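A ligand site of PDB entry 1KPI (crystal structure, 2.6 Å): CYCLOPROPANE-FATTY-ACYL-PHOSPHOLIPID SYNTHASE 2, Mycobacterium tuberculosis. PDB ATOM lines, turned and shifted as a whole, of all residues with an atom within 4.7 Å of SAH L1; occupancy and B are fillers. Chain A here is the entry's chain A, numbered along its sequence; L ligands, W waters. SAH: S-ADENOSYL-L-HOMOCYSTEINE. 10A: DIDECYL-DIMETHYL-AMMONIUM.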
ATOM      1  N   PRO A  15     -11.855 -18.030   4.808  1.00  0.00           N
ATOM      2  CA  PRO A  15     -11.838 -16.775   5.569  1.00  0.00           C
ATOM      3  C   PRO A  15     -12.443 -16.883   6.982  1.00  0.00           C
ATOM      4  O   PRO A  15     -13.404 -17.630   7.203  1.00  0.00           O
ATOM      5  CB  PRO A  15     -12.619 -15.819   4.679  1.00  0.00           C
ATOM      6  CG  PRO A  15     -12.293 -16.332   3.302  1.00  0.00           C
ATOM      7  CD  PRO A  15     -12.425 -17.825   3.472  1.00  0.00           C
ATOM      8  N   PRO A  16     -11.889 -16.141   7.958  1.00  0.00           N
ATOM      9  CA  PRO A  16     -12.356 -16.120   9.353  1.00  0.00           C
ATOM     10  C   PRO A  16     -13.542 -15.175   9.489  1.00  0.00           C
ATOM     11  O   PRO A  16     -13.412 -14.114  10.104  1.00  0.00           O
ATOM     12  CB  PRO A  16     -11.147 -15.596  10.122  1.00  0.00           C
ATOM     13  CG  PRO A  16     -10.005 -15.590   9.122  1.00  0.00           C
ATOM     14  CD  PRO A  16     -10.658 -15.341   7.822  1.00  0.00           C
ATOM     15  N   VAL A  20     -13.991 -12.424  12.546  1.00  0.00           N
ATOM     16  CA  VAL A  20     -13.851 -11.040  12.138  1.00  0.00           C
ATOM     17  C   VAL A  20     -15.111 -10.218  12.408  1.00  0.00           C
ATOM     18  O   VAL A  20     -15.037  -9.101  12.917  1.00  0.00           O
ATOM     19  CB  VAL A  20     -13.465 -10.939  10.651  1.00  0.00           C
ATOM     20  CG1 VAL A  20     -13.480  -9.484  10.192  1.00  0.00           C
ATOM     21  CG2 VAL A  20     -12.083 -11.528  10.438  1.00  0.00           C
ATOM     22  N   TYR A  24     -15.786  -6.204  14.192  1.00  0.00           N
ATOM     23  CA  TYR A  24     -16.162  -5.163  13.244  1.00  0.00           C
ATOM     24  C   TYR A  24     -17.613  -4.893  12.931  1.00  0.00           C
ATOM     25  O   TYR A  24     -17.930  -3.859  12.363  1.00  0.00           O
ATOM     26  CB  TYR A  24     -15.385  -5.367  11.956  1.00  0.00           C
ATOM     27  CG  TYR A  24     -13.903  -5.422  12.190  1.00  0.00           C
ATOM     28  CD1 TYR A  24     -13.207  -6.624  12.079  1.00  0.00           C
ATOM     29  CD2 TYR A  24     -13.203  -4.280  12.610  1.00  0.00           C
ATOM     30  CE1 TYR A  24     -11.848  -6.697  12.377  1.00  0.00           C
ATOM     31  CE2 TYR A  24     -11.834  -4.351  12.909  1.00  0.00           C
ATOM     32  CZ  TYR A  24     -11.166  -5.563  12.787  1.00  0.00           C
ATOM     33  OH  TYR A  24      -9.831  -5.669  13.095  1.00  0.00           O
ATOM     34  N   MET A  39     -13.110   7.381  10.110  1.00  0.00           N
ATOM     35  CA  MET A  39     -13.230   6.039  10.689  1.00  0.00           C
ATOM     36  C   MET A  39     -12.068   5.126  10.352  1.00  0.00           C
ATOM     37  O   MET A  39     -12.258   3.918  10.175  1.00  0.00           O
ATOM     38  CB  MET A  39     -14.532   5.368  10.244  1.00  0.00           C
ATOM     39  CG  MET A  39     -15.765   6.089  10.731  1.00  0.00           C
ATOM     40  SD  MET A  39     -17.279   5.268  10.259  1.00  0.00           S
ATOM     41  CE  MET A  39     -17.453   4.030  11.613  1.00  0.00           C
ATOM     42  N   THR A  40     -10.873   5.706  10.231  1.00  0.00           N
ATOM     43  CA  THR A  40      -9.662   4.933   9.945  1.00  0.00           C
ATOM     44  C   THR A  40      -9.387   4.157  11.230  1.00  0.00           C
ATOM     45  O   THR A  40      -9.300   4.752  12.301  1.00  0.00           O
ATOM     46  CB  THR A  40      -8.498   5.854   9.654  1.00  0.00           C
ATOM     47  OG1 THR A  40      -8.854   6.708   8.565  1.00  0.00           O
ATOM     48  CG2 THR A  40      -7.248   5.063   9.305  1.00  0.00           C
ATOM     49  N   TYR A  41      -9.253   2.850  11.119  1.00  0.00           N
ATOM     50  CA  TYR A  41      -9.070   2.011  12.296  1.00  0.00           C
ATOM     51  C   TYR A  41      -7.741   1.248  12.348  1.00  0.00           C
ATOM     52  O   TYR A  41      -7.713   0.034  12.456  1.00  0.00           O
ATOM     53  CB  TYR A  41     -10.267   1.066  12.385  1.00  0.00           C
ATOM     54  CG  TYR A  41     -10.468   0.348  13.706  1.00  0.00           C
ATOM     55  CD1 TYR A  41     -10.030   0.889  14.916  1.00  0.00           C
ATOM     56  CD2 TYR A  41     -11.175  -0.858  13.743  1.00  0.00           C
ATOM     57  CE1 TYR A  41     -10.313   0.248  16.141  1.00  0.00           C
ATOM     58  CE2 TYR A  41     -11.455  -1.506  14.949  1.00  0.00           C
ATOM     59  CZ  TYR A  41     -11.029  -0.952  16.141  1.00  0.00           C
ATOM     60  OH  TYR A  41     -11.328  -1.598  17.311  1.00  0.00           O
ATOM     61  N   SER A  42      -6.644   1.991  12.268  1.00  0.00           N
ATOM     62  CA  SER A  42      -5.315   1.410  12.337  1.00  0.00           C
ATOM     63  C   SER A  42      -4.364   2.509  12.833  1.00  0.00           C
ATOM     64  O   SER A  42      -4.743   3.686  12.872  1.00  0.00           O
ATOM     65  CB  SER A  42      -4.880   0.866  10.967  1.00  0.00           C
ATOM     66  OG  SER A  42      -4.984   1.856   9.960  1.00  0.00           O
ATOM     67  N   ASP A  78      -7.253  -2.791  -1.945  1.00  0.00           N
ATOM     68  CA  ASP A  78      -7.158  -2.539  -0.512  1.00  0.00           C
ATOM     69  C   ASP A  78      -7.638  -3.818   0.194  1.00  0.00           C
ATOM     70  O   ASP A  78      -8.843  -4.091   0.238  1.00  0.00           O
ATOM     71  CB  ASP A  78      -8.053  -1.354  -0.143  1.00  0.00           C
ATOM     72  CG  ASP A  78      -8.030  -1.016   1.343  1.00  0.00           C
ATOM     73  OD1 ASP A  78      -7.608  -1.858   2.167  1.00  0.00           O
ATOM     74  OD2 ASP A  78      -8.452   0.123   1.682  1.00  0.00           O
ATOM     75  N   ILE A  79      -6.713  -4.614   0.719  1.00  0.00           N
ATOM     76  CA  ILE A  79      -7.086  -5.860   1.406  1.00  0.00           C
ATOM     77  C   ILE A  79      -7.480  -5.579   2.863  1.00  0.00           C
ATOM     78  O   ILE A  79      -6.629  -5.323   3.704  1.00  0.00           O
ATOM     79  CB  ILE A  79      -5.922  -6.883   1.383  1.00  0.00           C
ATOM     80  CG1 ILE A  79      -5.533  -7.193  -0.063  1.00  0.00           C
ATOM     81  CG2 ILE A  79      -6.342  -8.159   2.097  1.00  0.00           C
ATOM     82  CD1 ILE A  79      -4.308  -8.079  -0.205  1.00  0.00           C
ATOM     83  N   GLY A  80      -8.775  -5.656   3.153  1.00  0.00           N
ATOM     84  CA  GLY A  80      -9.262  -5.384   4.501  1.00  0.00           C
ATOM     85  C   GLY A  80      -9.428  -3.880   4.596  1.00  0.00           C
ATOM     86  O   GLY A  80      -8.752  -3.217   5.383  1.00  0.00           O
ATOM     87  N   CYS A  81     -10.360  -3.350   3.805  1.00  0.00           N
ATOM     88  CA  CYS A  81     -10.622  -1.909   3.715  1.00  0.00           C
ATOM     89  C   CYS A  81     -11.420  -1.218   4.832  1.00  0.00           C
ATOM     90  O   CYS A  81     -11.711  -0.026   4.737  1.00  0.00           O
ATOM     91  CB  CYS A  81     -11.307  -1.640   2.370  1.00  0.00           C
ATOM     92  SG  CYS A  81     -12.861  -2.562   2.201  1.00  0.00           S
ATOM     93  N   GLY A  82     -11.793  -1.953   5.874  1.00  0.00           N
ATOM     94  CA  GLY A  82     -12.540  -1.351   6.968  1.00  0.00           C
ATOM     95  C   GLY A  82     -13.646  -0.403   6.520  1.00  0.00           C
ATOM     96  O   GLY A  82     -14.487  -0.766   5.711  1.00  0.00           O
ATOM     97  N   SER A  85     -11.877   4.626   4.237  1.00  0.00           N
ATOM     98  CA  SER A  85     -11.003   5.791   4.134  1.00  0.00           C
ATOM     99  C   SER A  85      -9.853   5.676   3.106  1.00  0.00           C
ATOM    100  O   SER A  85      -9.628   6.594   2.306  1.00  0.00           O
ATOM    101  CB  SER A  85     -10.406   6.112   5.507  1.00  0.00           C
ATOM    102  OG  SER A  85      -9.530   5.095   5.947  1.00  0.00           O
ATOM    103  N   LEU A 101     -11.606  -5.126  -0.189  1.00  0.00           N
ATOM    104  CA  LEU A 101     -11.996  -6.404   0.401  1.00  0.00           C
ATOM    105  C   LEU A 101     -12.266  -6.288   1.908  1.00  0.00           C
ATOM    106  O   LEU A 101     -11.522  -5.638   2.634  1.00  0.00           O
ATOM    107  CB  LEU A 101     -10.898  -7.436   0.176  1.00  0.00           C
ATOM    108  CG  LEU A 101     -10.818  -8.215  -1.123  1.00  0.00           C
ATOM    109  CD1 LEU A 101     -11.155  -7.328  -2.299  1.00  0.00           C
ATOM    110  CD2 LEU A 101      -9.428  -8.822  -1.252  1.00  0.00           C
ATOM    111  N   THR A 102     -13.325  -6.942   2.370  1.00  0.00           N
ATOM    112  CA  THR A 102     -13.669  -6.932   3.788  1.00  0.00           C
ATOM    113  C   THR A 102     -14.633  -8.073   4.096  1.00  0.00           C
ATOM    114  O   THR A 102     -15.294  -8.581   3.197  1.00  0.00           O
ATOM    115  CB  THR A 102     -14.320  -5.606   4.204  1.00  0.00           C
ATOM    116  OG1 THR A 102     -14.697  -5.670   5.591  1.00  0.00           O
ATOM    117  CG2 THR A 102     -15.562  -5.333   3.358  1.00  0.00           C
ATOM    118  N   LEU A 103     -14.699  -8.495   5.355  1.00  0.00           N
ATOM    119  CA  LEU A 103     -15.589  -9.573   5.726  1.00  0.00           C
ATOM    120  C   LEU A 103     -16.723  -9.001   6.579  1.00  0.00           C
ATOM    121  O   LEU A 103     -17.651  -9.716   6.966  1.00  0.00           O
ATOM    122  CB  LEU A 103     -14.841 -10.636   6.534  1.00  0.00           C
ATOM    123  CG  LEU A 103     -13.639 -11.362   5.914  1.00  0.00           C
ATOM    124  CD1 LEU A 103     -13.115 -12.397   6.915  1.00  0.00           C
ATOM    125  CD2 LEU A 103     -14.050 -12.047   4.612  1.00  0.00           C
ATOM    126  N   SER A 104     -16.641  -7.704   6.857  1.00  0.00           N
ATOM    127  CA  SER A 104     -17.649  -7.032   7.657  1.00  0.00           C
ATOM    128  C   SER A 104     -18.868  -6.590   6.836  1.00  0.00           C
ATOM    129  O   SER A 104     -18.736  -6.006   5.751  1.00  0.00           O
ATOM    130  CB  SER A 104     -17.023  -5.822   8.354  1.00  0.00           C
ATOM    131  OG  SER A 104     -18.011  -5.062   9.037  1.00  0.00           O
ATOM    132  N   GLN A 107     -19.337  -2.632   7.416  1.00  0.00           N
ATOM    133  CA  GLN A 107     -18.337  -1.862   6.705  1.00  0.00           C
ATOM    134  C   GLN A 107     -18.723  -1.845   5.231  1.00  0.00           C
ATOM    135  O   GLN A 107     -18.610  -0.822   4.548  1.00  0.00           O
ATOM    136  CB  GLN A 107     -16.938  -2.469   6.891  1.00  0.00           C
ATOM    137  CG  GLN A 107     -16.550  -2.587   8.360  1.00  0.00           C
ATOM    138  CD  GLN A 107     -15.088  -2.970   8.578  1.00  0.00           C
ATOM    139  OE1 GLN A 107     -14.541  -3.821   7.875  1.00  0.00           O
ATOM    140  NE2 GLN A 107     -14.467  -2.359   9.583  1.00  0.00           N
ATOM    141  N   GLN A 129     -15.619 -10.160   0.425  1.00  0.00           N
ATOM    142  CA  GLN A 129     -14.815 -11.263  -0.076  1.00  0.00           C
ATOM    143  C   GLN A 129     -13.433 -11.327   0.601  1.00  0.00           C
ATOM    144  O   GLN A 129     -12.712 -10.315   0.675  1.00  0.00           O
ATOM    145  CB  GLN A 129     -14.664 -11.110  -1.597  1.00  0.00           C
ATOM    146  CG  GLN A 129     -13.595 -11.969  -2.240  1.00  0.00           C
ATOM    147  CD  GLN A 129     -13.438 -11.706  -3.737  1.00  0.00           C
ATOM    148  OE1 GLN A 129     -13.501 -10.556  -4.193  1.00  0.00           O
ATOM    149  NE2 GLN A 129     -13.210 -12.764  -4.505  1.00  0.00           N
ATOM    150  N   GLY A 130     -13.056 -12.511   1.074  1.00  0.00           N
ATOM    151  CA  GLY A 130     -11.762 -12.679   1.725  1.00  0.00           C
ATOM    152  C   GLY A 130     -10.605 -12.704   0.750  1.00  0.00           C
ATOM    153  O   GLY A 130     -10.770 -13.041  -0.433  1.00  0.00           O
ATOM    154  N   TRP A 131      -9.411 -12.349   1.226  1.00  0.00           N
ATOM    155  CA  TRP A 131      -8.236 -12.352   0.375  1.00  0.00           C
ATOM    156  C   TRP A 131      -7.980 -13.757  -0.157  1.00  0.00           C
ATOM    157  O   TRP A 131      -7.389 -13.931  -1.235  1.00  0.00           O
ATOM    158  CB  TRP A 131      -6.994 -11.885   1.150  1.00  0.00           C
ATOM    159  CG  TRP A 131      -6.552 -12.775   2.299  1.00  0.00           C
ATOM    160  CD1 TRP A 131      -6.875 -12.644   3.629  1.00  0.00           C
ATOM    161  CD2 TRP A 131      -5.687 -13.914   2.211  1.00  0.00           C
ATOM    162  NE1 TRP A 131      -6.245 -13.613   4.371  1.00  0.00           N
ATOM    163  CE2 TRP A 131      -5.516 -14.409   3.534  1.00  0.00           C
ATOM    164  CE3 TRP A 131      -5.026 -14.561   1.153  1.00  0.00           C
ATOM    165  CZ2 TRP A 131      -4.711 -15.525   3.818  1.00  0.00           C
ATOM    166  CZ3 TRP A 131      -4.222 -15.674   1.447  1.00  0.00           C
ATOM    167  CH2 TRP A 131      -4.067 -16.140   2.767  1.00  0.00           C
ATOM    168  N   GLU A 132      -8.421 -14.756   0.598  1.00  0.00           N
ATOM    169  CA  GLU A 132      -8.240 -16.153   0.225  1.00  0.00           C
ATOM    170  C   GLU A 132      -8.987 -16.524  -1.043  1.00  0.00           C
ATOM    171  O   GLU A 132      -8.659 -17.508  -1.705  1.00  0.00           O
ATOM    172  CB  GLU A 132      -8.702 -17.075   1.359  1.00  0.00           C
ATOM    173  CG  GLU A 132      -7.906 -16.944   2.663  1.00  0.00           C
ATOM    174  CD  GLU A 132      -8.593 -16.077   3.707  1.00  0.00           C
ATOM    175  OE1 GLU A 132      -8.248 -16.197   4.900  1.00  0.00           O
ATOM    176  OE2 GLU A 132      -9.477 -15.284   3.341  1.00  0.00           O
ATOM    177  N   LEU A 144      -3.731  -2.290   5.487  1.00  0.00           N
ATOM    178  CA  LEU A 144      -3.426  -1.627   6.760  1.00  0.00           C
ATOM    179  C   LEU A 144      -4.214  -2.231   7.905  1.00  0.00           C
ATOM    180  O   LEU A 144      -5.439  -2.083   7.966  1.00  0.00           O
ATOM    181  CB  LEU A 144      -3.771  -0.134   6.670  1.00  0.00           C
ATOM    182  CG  LEU A 144      -3.358   0.670   5.434  1.00  0.00           C
ATOM    183  CD1 LEU A 144      -4.069   2.007   5.479  1.00  0.00           C
ATOM    184  CD2 LEU A 144      -1.857   0.852   5.383  1.00  0.00           C
ATOM    185  N   GLY A 145      -3.525  -2.907   8.824  1.00  0.00           N
ATOM    186  CA  GLY A 145      -4.186  -3.484   9.977  1.00  0.00           C
ATOM    187  C   GLY A 145      -5.167  -4.619   9.750  1.00  0.00           C
ATOM    188  O   GLY A 145      -6.100  -4.819  10.533  1.00  0.00           O
ATOM    189  N   ALA A 146      -4.953  -5.377   8.680  1.00  0.00           N
ATOM    190  CA  ALA A 146      -5.829  -6.508   8.391  1.00  0.00           C
ATOM    191  C   ALA A 146      -5.017  -7.793   8.503  1.00  0.00           C
ATOM    192  O   ALA A 146      -5.556  -8.857   8.803  1.00  0.00           O
ATOM    193  CB  ALA A 146      -6.409  -6.373   6.994  1.00  0.00           C
ATOM    194  N   HIS A 149      -5.179 -10.666  11.101  1.00  0.00           N
ATOM    195  CA  HIS A 149      -6.265 -11.647  11.026  1.00  0.00           C
ATOM    196  C   HIS A 149      -5.938 -12.762  10.024  1.00  0.00           C
ATOM    197  O   HIS A 149      -6.540 -13.835  10.068  1.00  0.00           O
ATOM    198  CB  HIS A 149      -7.566 -10.986  10.583  1.00  0.00           C
ATOM    199  CG  HIS A 149      -8.210 -10.127  11.615  1.00  0.00           C
ATOM    200  ND1 HIS A 149      -8.694 -10.632  12.811  1.00  0.00           N
ATOM    201  CD2 HIS A 149      -8.496  -8.800  11.631  1.00  0.00           C
ATOM    202  CE1 HIS A 149      -9.239  -9.652  13.507  1.00  0.00           C
ATOM    203  NE2 HIS A 149      -9.135  -8.535  12.818  1.00  0.00           N
ATOM    204  N   PHE A 150      -4.980 -12.503   9.136  1.00  0.00           N
ATOM    205  CA  PHE A 150      -4.623 -13.450   8.073  1.00  0.00           C
ATOM    206  C   PHE A 150      -4.093 -14.839   8.433  1.00  0.00           C
ATOM    207  O   PHE A 150      -4.147 -15.757   7.600  1.00  0.00           O
ATOM    208  CB  PHE A 150      -3.658 -12.768   7.087  1.00  0.00           C
ATOM    209  CG  PHE A 150      -4.267 -11.572   6.379  1.00  0.00           C
ATOM    210  CD1 PHE A 150      -5.568 -11.147   6.690  1.00  0.00           C
ATOM    211  CD2 PHE A 150      -3.543 -10.871   5.415  1.00  0.00           C
ATOM    212  CE1 PHE A 150      -6.132 -10.043   6.057  1.00  0.00           C
ATOM    213  CE2 PHE A 150      -4.097  -9.759   4.769  1.00  0.00           C
ATOM    214  CZ  PHE A 150      -5.407  -9.342   5.092  1.00  0.00           C
HETATM  215  N   SAH L   1      -7.615  -1.115   6.753  1.00  0.00           N
HETATM  216  CA  SAH L   1      -8.735  -0.458   7.433  1.00  0.00           C
HETATM  217  CB  SAH L   1      -9.463  -1.387   8.432  1.00  0.00           C
HETATM  218  CG  SAH L   1      -8.616  -2.320   9.323  1.00  0.00           C
HETATM  219  SD  SAH L   1      -9.625  -3.316  10.446  1.00  0.00           S
HETATM  220  C   SAH L   1      -8.268   0.815   8.169  1.00  0.00           C
HETATM  221  O   SAH L   1      -7.049   1.031   8.247  1.00  0.00           O
HETATM  222  OXT SAH L   1      -9.141   1.573   8.664  1.00  0.00           O
HETATM  223  C5' SAH L   1      -9.323  -5.000   9.803  1.00  0.00           C
HETATM  224  C4' SAH L   1      -9.978  -5.197   8.437  1.00  0.00           C
HETATM  225  O4' SAH L   1      -9.504  -6.365   7.716  1.00  0.00           O
HETATM  226  C3' SAH L   1     -11.503  -5.322   8.505  1.00  0.00           C
HETATM  227  O3' SAH L   1     -12.122  -4.430   7.545  1.00  0.00           O
HETATM  228  C2' SAH L   1     -11.763  -6.789   8.212  1.00  0.00           C
HETATM  229  O2' SAH L   1     -13.056  -6.978   7.625  1.00  0.00           O
HETATM  230  C1' SAH L   1     -10.640  -7.142   7.283  1.00  0.00           C
HETATM  231  N9  SAH L   1     -10.308  -8.576   7.229  1.00  0.00           N
HETATM  232  C8  SAH L   1     -10.041  -9.464   8.222  1.00  0.00           C
HETATM  233  N7  SAH L   1      -9.774 -10.687   7.859  1.00  0.00           N
HETATM  234  C5  SAH L   1      -9.872 -10.609   6.482  1.00  0.00           C
HETATM  235  C6  SAH L   1      -9.696 -11.645   5.340  1.00  0.00           C
HETATM  236  N6  SAH L   1      -9.362 -12.933   5.555  1.00  0.00           N
HETATM  237  N1  SAH L   1      -9.885 -11.177   4.068  1.00  0.00           N
HETATM  238  C2  SAH L   1     -10.214  -9.870   3.868  1.00  0.00           C
HETATM  239  N3  SAH L   1     -10.394  -8.886   4.781  1.00  0.00           N
HETATM  240  C4  SAH L   1     -10.213  -9.326   6.073  1.00  0.00           C
HETATM  241  C1  10A L   2      -1.737 -11.131  21.290  1.00  0.00           C
HETATM  242  C2  10A L   2      -3.052 -11.354  20.528  1.00  0.00           C
HETATM  243  C3  10A L   2      -3.183 -10.269  19.470  1.00  0.00           C
HETATM  244  C4  10A L   2      -4.446 -10.320  18.595  1.00  0.00           C
HETATM  245  C5  10A L   2      -4.297  -9.102  17.679  1.00  0.00           C
HETATM  246  C6  10A L   2      -5.493  -8.877  16.750  1.00  0.00           C
HETATM  247  C7  10A L   2      -5.170  -7.541  16.063  1.00  0.00           C
HETATM  248  C8  10A L   2      -6.343  -6.982  15.268  1.00  0.00           C
HETATM  249  C9  10A L   2      -5.858  -5.580  14.851  1.00  0.00           C
HETATM  250  C10 10A L   2      -7.022  -4.767  14.317  1.00  0.00           C
HETATM  251  N1  10A L   2      -6.901  -3.255  14.094  1.00  0.00           N
HETATM  252  C11 10A L   2      -8.293  -2.804  13.688  1.00  0.00           C
HETATM  253  C12 10A L   2      -5.970  -2.935  12.940  1.00  0.00           C
HETATM  254  C13 10A L   2      -6.398  -2.377  15.237  1.00  0.00           C
HETATM  255  C14 10A L   2      -7.029  -2.320  16.658  1.00  0.00           C
HETATM  256  C15 10A L   2      -6.227  -1.448  17.654  1.00  0.00           C
HETATM  257  C16 10A L   2      -4.847  -2.001  18.109  1.00  0.00           C
HETATM  258  C17 10A L   2      -4.931  -3.270  18.979  1.00  0.00           C
HETATM  259  C18 10A L   2      -3.524  -3.772  19.332  1.00  0.00           C
HETATM  260  C19 10A L   2      -3.645  -5.013  20.208  1.00  0.00           C
HETATM  261  C20 10A L   2      -2.246  -5.532  20.577  1.00  0.00           C
HETATM  262  C21 10A L   2      -2.417  -6.742  21.498  1.00  0.00           C
HETATM  263  C22 10A L   2      -1.040  -7.302  21.858  1.00  0.00           C
HETATM  264  O   HOH W   1      -6.459  -2.627   4.611  1.00  0.00           O
HETATM  265  O   HOH W   2      -7.441   0.674   4.556  1.00  0.00           O
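Water W2 bridges a nitrogen (N) of SAH L1 (2.8 Å) and the side-chain carboxylate of Asp 78 (3.1 Å).
The side-chain amide oxygen (OE1) of Gln 107 lies within hydrogen-bond range of an oxygen (O3') of SAH L1 (2.5 Å). The backbone carbonyl oxygen (O) of Leu 144 lies within hydrogen-bond range of a nitrogen (N) of SAH L1 (2.7 Å). O of Gly 80 is in hydrogen-bond range of N of SAH L1. OXT of SAH L1 is in hydrogen-bond range of N of Tyr 41 (2.8 Å). An oxygen (O) of SAH L1 lies within hydrogen-bond range of the side-chain hydroxyl (OG) of Ser 42 (2.8 Å). OG1 of Thr 102 is in hydrogen-bond range of O2' of SAH L1 (2.9 Å). The backbone NH (N) of Gly 82 sits at hydrogen-bond distance from an oxygen (O3') of SAH L1, at 3.0 Å. The backbone NH (N) of Trp 131 lies within hydrogen-bond range of a nitrogen (N1) of SAH L1, 3.1 Å away. The backbone NH (N) of Leu 103 lies within hydrogen-bond range of an oxygen (O2') of SAH L1 (3.2 Å). The side-chain carboxylate (OE2) of Glu 132 is in hydrogen-bond range of a nitrogen (N6) of SAH L1 (3.2 Å). The side-chain hydroxyl (OH) of Tyr 24 sits close to a sulfur (SD) of SAH L1.
The side-chain hydroxyl (OG1) of Thr 102 is in hydrogen-bond range of the side-chain amide oxygen (OE1) of Gln 107 (2.9 Å). The side-chain hydroxyl of Ser 104 lies close to the backbone NH of Gln 107, 3.2 Å away. N of Gly 80 lies within hydrogen-bond range of O of Leu 101. O of Thr 102 sits at hydrogen-bond distance from N of Gln 129, 3.2 Å away. The side-chain carboxylate of Glu 132 lies within hydrogen-bond range of the indole nitrogen of Trp 131, 3.3 Å away. A ring nitrogen (NE2) of His 149 is in hydrogen-bond range of the side-chain hydroxyl (OH) of Tyr 24 (3.0 Å). The side-chain hydroxyl (OG) of Ser 85 is in hydrogen-bond range of the side-chain hydroxyl (OG1) of Thr 40 (3.1 Å). The backbone NH (N) of Cys 81 lies within hydrogen-bond range of the backbone carbonyl oxygen (O) of Leu 101 (2.8 Å).
Merely in contact with SAH L1: Ala 146 (3.2 Å), Gly 145 (3.3 Å), Gly 130 (3.4 Å), His 149 (3.5 Å), Pro 16 (3.6 Å), Val 20 (3.6 Å), Thr 40 (3.6 Å), Ser 104 (3.7 Å), Phe 150 (3.8 Å) and Cys 81 (3.8 Å). Hydrophobic or aromatic side chains within 4 Å of SAH L1: Pro 16, Val 20, Tyr 24, Tyr 41, Leu 103, Trp 131, Leu 144, Ala 146, His 149 and Phe 150. Of the 28 residues printed, 21 come within 4 Å of SAH L1.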
